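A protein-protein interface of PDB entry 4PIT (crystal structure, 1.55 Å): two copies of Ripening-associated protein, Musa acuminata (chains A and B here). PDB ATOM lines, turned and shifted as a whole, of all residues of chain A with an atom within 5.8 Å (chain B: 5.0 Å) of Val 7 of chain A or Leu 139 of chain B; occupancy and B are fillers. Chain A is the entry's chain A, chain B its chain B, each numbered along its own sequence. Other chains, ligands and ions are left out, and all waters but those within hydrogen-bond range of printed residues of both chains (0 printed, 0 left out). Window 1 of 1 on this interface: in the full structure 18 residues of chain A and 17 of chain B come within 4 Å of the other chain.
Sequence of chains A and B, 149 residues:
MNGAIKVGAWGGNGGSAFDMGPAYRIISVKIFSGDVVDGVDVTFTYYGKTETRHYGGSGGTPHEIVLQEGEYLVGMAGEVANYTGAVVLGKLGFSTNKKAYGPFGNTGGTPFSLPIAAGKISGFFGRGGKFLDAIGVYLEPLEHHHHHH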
ATOM      1  N   ILE A   5      -2.785   5.634  23.601  1.00  0.00           N
ATOM      2  CA  ILE A   5      -1.380   5.966  23.832  1.00  0.00           C
ATOM      3  C   ILE A   5      -1.098   5.877  25.306  1.00  0.00           C
ATOM      4  O   ILE A   5      -1.682   6.633  26.080  1.00  0.00           O
ATOM      5  CB  ILE A   5      -0.959   7.368  23.301  1.00  0.00           C
ATOM      6  CG1 ILE A   5      -1.270   7.538  21.796  1.00  0.00           C
ATOM      7  CG2 ILE A   5       0.523   7.639  23.661  1.00  0.00           C
ATOM      8  CD1 ILE A   5      -0.417   6.690  20.932  1.00  0.00           C
ATOM      9  N   LYS A   6      -0.256   4.938  25.694  1.00  0.00           N
ATOM     10  CA  LYS A   6       0.119   4.733  27.086  1.00  0.00           C
ATOM     11  C   LYS A   6       1.619   4.790  27.207  1.00  0.00           C
ATOM     12  O   LYS A   6       2.322   3.988  26.570  1.00  0.00           O
ATOM     13  CB  LYS A   6      -0.402   3.391  27.616  1.00  0.00           C
ATOM     14  CG  LYS A   6      -1.929   3.322  27.644  1.00  0.00           C
ATOM     15  CD  LYS A   6      -2.452   1.899  27.983  1.00  0.00           C
ATOM     16  CE  LYS A   6      -2.195   1.486  29.416  1.00  0.00           C
ATOM     17  NZ  LYS A   6      -2.784   0.123  29.704  1.00  0.00           N
ATOM     18  N   VAL A   7       2.133   5.757  27.973  1.00  0.00           N
ATOM     19  CA  VAL A   7       3.584   5.855  28.164  1.00  0.00           C
ATOM     20  C   VAL A   7       3.911   5.578  29.624  1.00  0.00           C
ATOM     21  O   VAL A   7       3.111   5.859  30.516  1.00  0.00           O
ATOM     22  CB  VAL A   7       4.209   7.161  27.652  1.00  0.00           C
ATOM     23  CG1 VAL A   7       4.024   7.303  26.143  1.00  0.00           C
ATOM     24  CG2 VAL A   7       3.652   8.366  28.378  1.00  0.00           C
ATOM     25  N   GLY A   8       5.073   5.005  29.846  1.00  0.00           N
ATOM     26  CA  GLY A   8       5.433   4.485  31.152  1.00  0.00           C
ATOM     27  C   GLY A   8       5.103   2.998  31.132  1.00  0.00           C
ATOM     28  O   GLY A   8       4.961   2.405  30.047  1.00  0.00           O
ATOM     29  N   ALA A   9       5.000   2.338  32.288  1.00  0.00           N
ATOM     30  CA  ALA A   9       5.141   2.969  33.592  1.00  0.00           C
ATOM     31  C   ALA A   9       6.595   3.078  34.016  1.00  0.00           C
ATOM     32  O   ALA A   9       7.467   2.343  33.523  1.00  0.00           O
ATOM     33  CB  ALA A   9       4.381   2.131  34.636  1.00  0.00           C
ATOM     34  N   TRP A  10       6.847   4.029  34.917  1.00  0.00           N
ATOM     35  CA  TRP A  10       8.121   4.228  35.575  1.00  0.00           C
ATOM     36  C   TRP A  10       7.960   3.694  36.976  1.00  0.00           C
ATOM     37  O   TRP A  10       6.960   3.987  37.640  1.00  0.00           O
ATOM     38  CB  TRP A  10       8.513   5.722  35.612  1.00  0.00           C
ATOM     39  CG  TRP A  10       8.828   6.269  34.273  1.00  0.00           C
ATOM     40  CD1 TRP A  10      10.045   6.261  33.660  1.00  0.00           C
ATOM     41  CD2 TRP A  10       7.918   6.907  33.364  1.00  0.00           C
ATOM     42  NE1 TRP A  10       9.953   6.853  32.419  1.00  0.00           N
ATOM     43  CE2 TRP A  10       8.665   7.282  32.219  1.00  0.00           C
ATOM     44  CE3 TRP A  10       6.554   7.249  33.422  1.00  0.00           C
ATOM     45  CZ2 TRP A  10       8.091   7.995  31.139  1.00  0.00           C
ATOM     46  CZ3 TRP A  10       5.970   7.881  32.320  1.00  0.00           C
ATOM     47  CH2 TRP A  10       6.727   8.212  31.181  1.00  0.00           C
ATOM     48  N   LEU A 114       8.593  13.547  31.819  1.00  0.00           N
ATOM     49  CA  LEU A 114       7.743  13.437  30.646  1.00  0.00           C
ATOM     50  C   LEU A 114       7.133  14.783  30.314  1.00  0.00           C
ATOM     51  O   LEU A 114       5.990  15.070  30.687  1.00  0.00           O
ATOM     52  CB  LEU A 114       6.653  12.379  30.832  1.00  0.00           C
ATOM     53  CG  LEU A 114       5.739  12.192  29.600  1.00  0.00           C
ATOM     54  CD1 LEU A 114       6.411  11.353  28.538  1.00  0.00           C
ATOM     55  CD2 LEU A 114       4.402  11.583  30.014  1.00  0.00           C
ATOM     56  N   PHE A 125      -2.147   4.614  34.841  1.00  0.00           N
ATOM     57  CA  PHE A 125      -2.035   3.158  35.038  1.00  0.00           C
ATOM     58  C   PHE A 125      -0.744   2.926  35.778  1.00  0.00           C
ATOM     59  O   PHE A 125       0.061   3.855  35.922  1.00  0.00           O
ATOM     60  CB  PHE A 125      -2.095   2.364  33.727  1.00  0.00           C
ATOM     61  CG  PHE A 125      -0.918   2.587  32.809  1.00  0.00           C
ATOM     62  CD1 PHE A 125      -0.873   3.692  31.971  1.00  0.00           C
ATOM     63  CD2 PHE A 125       0.172   1.715  32.820  1.00  0.00           C
ATOM     64  CE1 PHE A 125       0.232   3.920  31.143  1.00  0.00           C
ATOM     65  CE2 PHE A 125       1.268   1.929  31.967  1.00  0.00           C
ATOM     66  CZ  PHE A 125       1.287   3.034  31.136  1.00  0.00           C
ATOM     67  N   ILE A 135       4.045   4.154  37.909  1.00  0.00           N
ATOM     68  CA  ILE A 135       2.978   4.971  37.353  1.00  0.00           C
ATOM     69  C   ILE A 135       3.275   5.277  35.905  1.00  0.00           C
ATOM     70  O   ILE A 135       4.427   5.521  35.536  1.00  0.00           O
ATOM     71  CB  ILE A 135       2.753   6.279  38.190  1.00  0.00           C
ATOM     72  CG1 ILE A 135       1.381   6.958  37.851  1.00  0.00           C
ATOM     73  CG2 ILE A 135       3.990   7.202  38.142  1.00  0.00           C
ATOM     74  CD1 ILE A 135       0.868   7.971  38.874  1.00  0.00           C
ATOM     75  N   GLY A 136       2.226   5.271  35.103  1.00  0.00           N
ATOM     76  CA  GLY A 136       2.276   5.659  33.709  1.00  0.00           C
ATOM     77  C   GLY A 136       1.036   6.458  33.372  1.00  0.00           C
ATOM     78  O   GLY A 136       0.139   6.642  34.214  1.00  0.00           O
ATOM     79  N   VAL A 137       1.010   6.998  32.162  1.00  0.00           N
ATOM     80  CA  VAL A 137      -0.112   7.841  31.775  1.00  0.00           C
ATOM     81  C   VAL A 137      -0.683   7.518  30.423  1.00  0.00           C
ATOM     82  O   VAL A 137       0.041   7.117  29.499  1.00  0.00           O
ATOM     83  CB  VAL A 137       0.287   9.351  31.788  1.00  0.00           C
ATOM     84  CG1 VAL A 137       0.515   9.864  33.217  1.00  0.00           C
ATOM     85  CG2 VAL A 137       1.517   9.609  30.924  1.00  0.00           C
ATOM     86  N   TYR A 138      -1.978   7.790  30.289  1.00  0.00           N
ATOM     87  CA  TYR A 138      -2.648   7.853  28.997  1.00  0.00           C
ATOM     88  C   TYR A 138      -2.469   9.256  28.446  1.00  0.00           C
ATOM     89  O   TYR A 138      -2.582  10.251  29.197  1.00  0.00           O
ATOM     90  CB  TYR A 138      -4.149   7.617  29.167  1.00  0.00           C
ATOM     91  CG  TYR A 138      -4.500   6.166  29.393  1.00  0.00           C
ATOM     92  CD1 TYR A 138      -4.472   5.616  30.671  1.00  0.00           C
ATOM     93  CD2 TYR A 138      -4.947   5.366  28.345  1.00  0.00           C
ATOM     94  CE1 TYR A 138      -4.790   4.272  30.889  1.00  0.00           C
ATOM     95  CE2 TYR A 138      -5.319   4.037  28.559  1.00  0.00           C
ATOM     96  CZ  TYR A 138      -5.260   3.503  29.838  1.00  0.00           C
ATOM     97  OH  TYR A 138      -5.605   2.187  30.075  1.00  0.00           O
ATOM     98  N   LEU A 139      -2.183   9.358  27.138  1.00  0.00           N
ATOM     99  CA  LEU A 139      -2.058  10.654  26.480  1.00  0.00           C
ATOM    100  C   LEU A 139      -3.115  10.824  25.436  1.00  0.00           C
ATOM    101  O   LEU A 139      -3.485   9.868  24.730  1.00  0.00           O
ATOM    102  CB  LEU A 139      -0.683  10.820  25.805  1.00  0.00           C
ATOM    103  CG  LEU A 139       0.539  10.746  26.747  1.00  0.00           C
ATOM    104  CD1 LEU A 139       1.842  10.846  25.949  1.00  0.00           C
ATOM    105  CD2 LEU A 139       0.471  11.778  27.874  1.00  0.00           C
ATOM    106  N   ILE B   5       0.533  13.915  18.933  1.00  0.00           N
ATOM    107  CA  ILE B   5       1.007  13.819  20.322  1.00  0.00           C
ATOM    108  C   ILE B   5       2.517  13.875  20.274  1.00  0.00           C
ATOM    109  O   ILE B   5       3.131  13.058  19.584  1.00  0.00           O
ATOM    110  CB  ILE B   5       0.494  12.569  21.034  1.00  0.00           C
ATOM    111  CG1 ILE B   5      -1.045  12.710  21.282  1.00  0.00           C
ATOM    112  CG2 ILE B   5       1.230  12.416  22.374  1.00  0.00           C
ATOM    113  CD1 ILE B   5      -1.712  11.509  21.812  1.00  0.00           C
ATOM    114  N   VAL B   7       6.004  14.190  22.698  1.00  0.00           N
ATOM    115  CA  VAL B   7       6.583  14.119  24.053  1.00  0.00           C
ATOM    116  C   VAL B   7       8.084  14.437  23.946  1.00  0.00           C
ATOM    117  O   VAL B   7       8.742  14.178  22.921  1.00  0.00           O
ATOM    118  CB  VAL B   7       6.303  12.788  24.796  1.00  0.00           C
ATOM    119  CG1 VAL B   7       4.807  12.603  25.050  1.00  0.00           C
ATOM    120  CG2 VAL B   7       6.870  11.602  24.049  1.00  0.00           C
ATOM    121  N   LEU B 114      11.756   6.697  27.994  1.00  0.00           N
ATOM    122  CA  LEU B 114      10.437   6.688  27.448  1.00  0.00           C
ATOM    123  C   LEU B 114       9.991   5.280  27.112  1.00  0.00           C
ATOM    124  O   LEU B 114      10.061   4.860  25.950  1.00  0.00           O
ATOM    125  CB  LEU B 114      10.306   7.631  26.232  1.00  0.00           C
ATOM    126  CG  LEU B 114       8.917   7.733  25.652  1.00  0.00           C
ATOM    127  CD1 LEU B 114       7.976   8.489  26.602  1.00  0.00           C
ATOM    128  CD2 LEU B 114       8.972   8.404  24.283  1.00  0.00           C
ATOM    129  N   PRO B 115       9.523   4.513  28.120  1.00  0.00           N
ATOM    130  CA  PRO B 115       8.890   3.226  27.810  1.00  0.00           C
ATOM    131  C   PRO B 115       7.498   3.498  27.250  1.00  0.00           C
ATOM    132  O   PRO B 115       6.840   4.414  27.715  1.00  0.00           O
ATOM    133  CB  PRO B 115       8.844   2.506  29.162  1.00  0.00           C
ATOM    134  CG  PRO B 115       9.109   3.507  30.176  1.00  0.00           C
ATOM    135  CD  PRO B 115       9.382   4.850  29.557  1.00  0.00           C
ATOM    136  N   ILE B 116       7.092   2.803  26.193  1.00  0.00           N
ATOM    137  CA  ILE B 116       5.783   3.028  25.580  1.00  0.00           C
ATOM    138  C   ILE B 116       4.987   1.729  25.751  1.00  0.00           C
ATOM    139  O   ILE B 116       5.224   0.747  25.039  1.00  0.00           O
ATOM    140  CB  ILE B 116       5.844   3.518  24.106  1.00  0.00           C
ATOM    141  CG1 ILE B 116       6.761   4.767  23.933  1.00  0.00           C
ATOM    142  CG2 ILE B 116       4.414   3.850  23.599  1.00  0.00           C
ATOM    143  CD1 ILE B 116       7.110   5.057  22.545  1.00  0.00           C
ATOM    144  N   ALA B 117       4.079   1.709  26.721  1.00  0.00           N
ATOM    145  CA  ALA B 117       3.260   0.527  26.989  1.00  0.00           C
ATOM    146  C   ALA B 117       2.308   0.246  25.822  1.00  0.00           C
ATOM    147  O   ALA B 117       2.022  -0.921  25.517  1.00  0.00           O
ATOM    148  CB  ALA B 117       2.472   0.703  28.279  1.00  0.00           C
ATOM    149  N   LYS B 120       3.715   3.728  19.422  1.00  0.00           N
ATOM    150  CA  LYS B 120       5.007   3.666  18.756  1.00  0.00           C
ATOM    151  C   LYS B 120       5.417   5.075  18.330  1.00  0.00           C
ATOM    152  O   LYS B 120       4.587   5.995  18.295  1.00  0.00           O
ATOM    153  CB  LYS B 120       4.952   2.738  17.526  1.00  0.00           C
ATOM    154  CG  LYS B 120       4.008   3.238  16.407  1.00  0.00           C
ATOM    155  CD  LYS B 120       4.055   2.231  15.233  1.00  0.00           C
ATOM    156  CE  LYS B 120       2.798   2.331  14.411  1.00  0.00           C
ATOM    157  NZ  LYS B 120       2.960   3.312  13.314  1.00  0.00           N
ATOM    158  N   ILE B 121       6.712   5.219  18.053  1.00  0.00           N
ATOM    159  CA  ILE B 121       7.260   6.499  17.602  1.00  0.00           C
ATOM    160  C   ILE B 121       6.972   6.675  16.139  1.00  0.00           C
ATOM    161  O   ILE B 121       7.264   5.767  15.332  1.00  0.00           O
ATOM    162  CB  ILE B 121       8.771   6.536  17.904  1.00  0.00           C
ATOM    163  CG1 ILE B 121       8.930   6.629  19.445  1.00  0.00           C
ATOM    164  CG2 ILE B 121       9.461   7.711  17.175  1.00  0.00           C
ATOM    165  CD1 ILE B 121      10.338   6.254  19.920  1.00  0.00           C
ATOM    166  N   SER B 122       6.454   7.863  15.769  1.00  0.00           N
ATOM    167  CA  SER B 122       6.136   8.101  14.365  1.00  0.00           C
ATOM    168  C   SER B 122       6.884   9.280  13.735  1.00  0.00           C
ATOM    169  O   SER B 122       6.659   9.572  12.551  1.00  0.00           O
ATOM    170  CB  SER B 122       4.638   8.342  14.222  1.00  0.00           C
ATOM    171  OG  SER B 122       4.245   9.444  15.022  1.00  0.00           O
ATOM    172  N   VAL B 137       9.806  13.012  20.438  1.00  0.00           N
ATOM    173  CA  VAL B 137       9.133  12.133  19.479  1.00  0.00           C
ATOM    174  C   VAL B 137       7.656  12.411  19.338  1.00  0.00           C
ATOM    175  O   VAL B 137       7.000  12.878  20.272  1.00  0.00           O
ATOM    176  CB  VAL B 137       9.323  10.626  19.854  1.00  0.00           C
ATOM    177  CG1 VAL B 137      10.775  10.175  19.680  1.00  0.00           C
ATOM    178  CG2 VAL B 137       8.823  10.295  21.246  1.00  0.00           C
ATOM    179  N   TYR B 138       7.144  12.113  18.152  1.00  0.00           N
ATOM    180  CA  TYR B 138       5.708  12.021  17.880  1.00  0.00           C
ATOM    181  C   TYR B 138       5.284  10.613  18.188  1.00  0.00           C
ATOM    182  O   TYR B 138       6.072   9.690  17.928  1.00  0.00           O
ATOM    183  CB  TYR B 138       5.387  12.310  16.414  1.00  0.00           C
ATOM    184  CG  TYR B 138       5.506  13.765  16.036  1.00  0.00           C
ATOM    185  CD1 TYR B 138       6.748  14.339  15.764  1.00  0.00           C
ATOM    186  CD2 TYR B 138       4.374  14.552  15.875  1.00  0.00           C
ATOM    187  CE1 TYR B 138       6.860  15.671  15.373  1.00  0.00           C
ATOM    188  CE2 TYR B 138       4.468  15.883  15.473  1.00  0.00           C
ATOM    189  CZ  TYR B 138       5.714  16.448  15.237  1.00  0.00           C
ATOM    190  OH  TYR B 138       5.796  17.772  14.866  1.00  0.00           O
ATOM    191  N   LEU B 139       4.036  10.418  18.698  1.00  0.00           N
ATOM    192  CA  LEU B 139       3.533   9.067  19.004  1.00  0.00           C
ATOM    193  C   LEU B 139       2.264   8.788  18.252  1.00  0.00           C
ATOM    194  O   LEU B 139       1.487   9.697  17.979  1.00  0.00           O
ATOM    195  CB  LEU B 139       3.217   8.953  20.517  1.00  0.00           C
ATOM    196  CG  LEU B 139       4.402   9.172  21.445  1.00  0.00           C
ATOM    197  CD1 LEU B 139       3.965   9.085  22.917  1.00  0.00           C
ATOM    198  CD2 LEU B 139       5.532   8.190  21.180  1.00  0.00           C
ATOM    199  N   GLU B 140       2.019   7.509  17.998  1.00  0.00           N
ATOM    200  CA  GLU B 140       0.756   7.064  17.417  1.00  0.00           C
ATOM    201  C   GLU B 140       0.482   5.665  17.946  1.00  0.00           C
ATOM    202  O   GLU B 140       1.377   5.023  18.495  1.00  0.00           O
ATOM    203  CB  GLU B 140       0.789   7.136  15.895  1.00  0.00           C
ATOM    204  CG  GLU B 140       1.555   6.071  15.173  1.00  0.00           C
ATOM    205  CD  GLU B 140       1.130   6.165  13.712  1.00  0.00           C
ATOM    206  OE1 GLU B 140       1.180   7.281  13.146  1.00  0.00           O
ATOM    207  OE2 GLU B 140       0.561   5.180  13.203  1.00  0.00           O
ATOM    208  N   PRO B 141      -0.776   5.208  17.920  1.00  0.00           N
ATOM    209  CA  PRO B 141      -1.071   3.871  18.455  1.00  0.00           C
ATOM    210  C   PRO B 141      -0.422   2.770  17.617  1.00  0.00           C
ATOM    211  O   PRO B 141      -0.046   2.983  16.468  1.00  0.00           O
ATOM    212  CB  PRO B 141      -2.608   3.796  18.382  1.00  0.00           C
ATOM    213  CG  PRO B 141      -3.066   5.199  18.308  1.00  0.00           C
ATOM    214  CD  PRO B 141      -1.995   5.886  17.456  1.00  0.00           C
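Among the printed residues, merely in contact across the chains: Ile 5 of chain A with Ile 5 of chain B (3.996 Å), Ile 5 of chain A with Leu 139 of chain B (3.8 Å), Ile 5 of chain A with Glu 140 of chain B (3.3 Å), Ile 5 of chain A with Pro 141 of chain B (3.4 Å), Lys 6 of chain A with Ile 116 of chain B (3.6 Å), Val 7 of chain A with Pro 115 of chain B (3.6 Å), Val 7 of chain A with Leu 139 of chain B (3.7 Å), Gly 8 of chain A with Ala 117 of chain B (3.5 Å), Ala 9 of chain A with Pro 115 of chain B (3.9 Å), Trp 10 of chain A with Pro 115 of chain B (3.5 Å), Leu 114 of chain A with Leu 114 of chain B (3.8 Å), Phe 125 of chain A with Ala 117 of chain B (3.9 Å), Leu 139 of chain A with Ile 5 of chain B (3.8 Å) and Leu 139 of chain A with Val 7 of chain B (3.6 Å).
Ile 5 of chain B touches its own counterpart, Ile 5 of chain A. Ile 5 of chain A touches Leu 139 of chain B, and with the chains exchanged Leu 139 of chain A touches Ile 5 of chain B. Val 7 of chain A touches Leu 139 of chain B, and with the chains exchanged Leu 139 of chain A touches Val 7 of chain B. Leu 114 of chain A touches its own counterpart, Leu 114 of chain B. Positions printed for both chains: 5, 7, 114, 137, 138 and 139. Of the 16 pairs that touch across the chains among the printed residues, 6 have their exchanged pair printed and touching as well.
Of the printed residues of chain B, Ile 5 of chain A touches Ile 5, Leu 139, Glu 140 and Pro 141. Printed residues of chain B within 4 Å of Lys 6 of chain A: Ile 116 and Ala 117. Of the printed residues of chain B, Val 7 of chain A touches Pro 115 and Leu 139. Val 137 of chain A touches none of the printed residues of chain B. Printed residues of chain A within 4 Å of Leu 139 of chain B: Ile 5 (3.8 Å) and Val 7 (3.7 Å).
The backbone carbonyl oxygen (O) of Ile 135 of chain A is in hydrogen-bond range of the backbone NH (N) of Trp 10 of chain A, at 2.9 Å. O of Val 137 of chain B sits at hydrogen-bond distance from N of Val 7 of chain B (2.9 Å). The backbone carbonyl oxygen (O) of Val 7 of chain A is in hydrogen-bond range of the backbone NH (N) of Val 137 of chain A (2.9 Å). O of Phe 125 of chain A lies within hydrogen-bond range of N of Gly 136 of chain A (2.7 Å). O of Ile 5 of chain B sits at hydrogen-bond distance from N of Leu 139 of chain B, at 2.9 Å. The backbone carbonyl oxygen (O) of Ile 5 of chain A lies within hydrogen-bond range of the backbone NH (N) of Leu 139 of chain A (3.0 Å).
Of the 14 printed residues of chain B, 9 touch a printed residue of chain A. Hydrophobic or aromatic side chains of chain A within 4 Å of the printed part of chain B: Ile 5, Val 7, Trp 10, Leu 114, Phe 125 and Leu 139. Among the printed residues, 16 pairs touch across the chains.
The backbone NH (N) of Gly 8 of chain A sits at hydrogen-bond distance from the backbone carbonyl oxygen (O) of Pro 115 of chain B (2.8 Å). The backbone NH (N) of Ala 117 of chain B sits at hydrogen-bond distance from the backbone carbonyl oxygen (O) of Lys 6 of chain A (2.9 Å).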
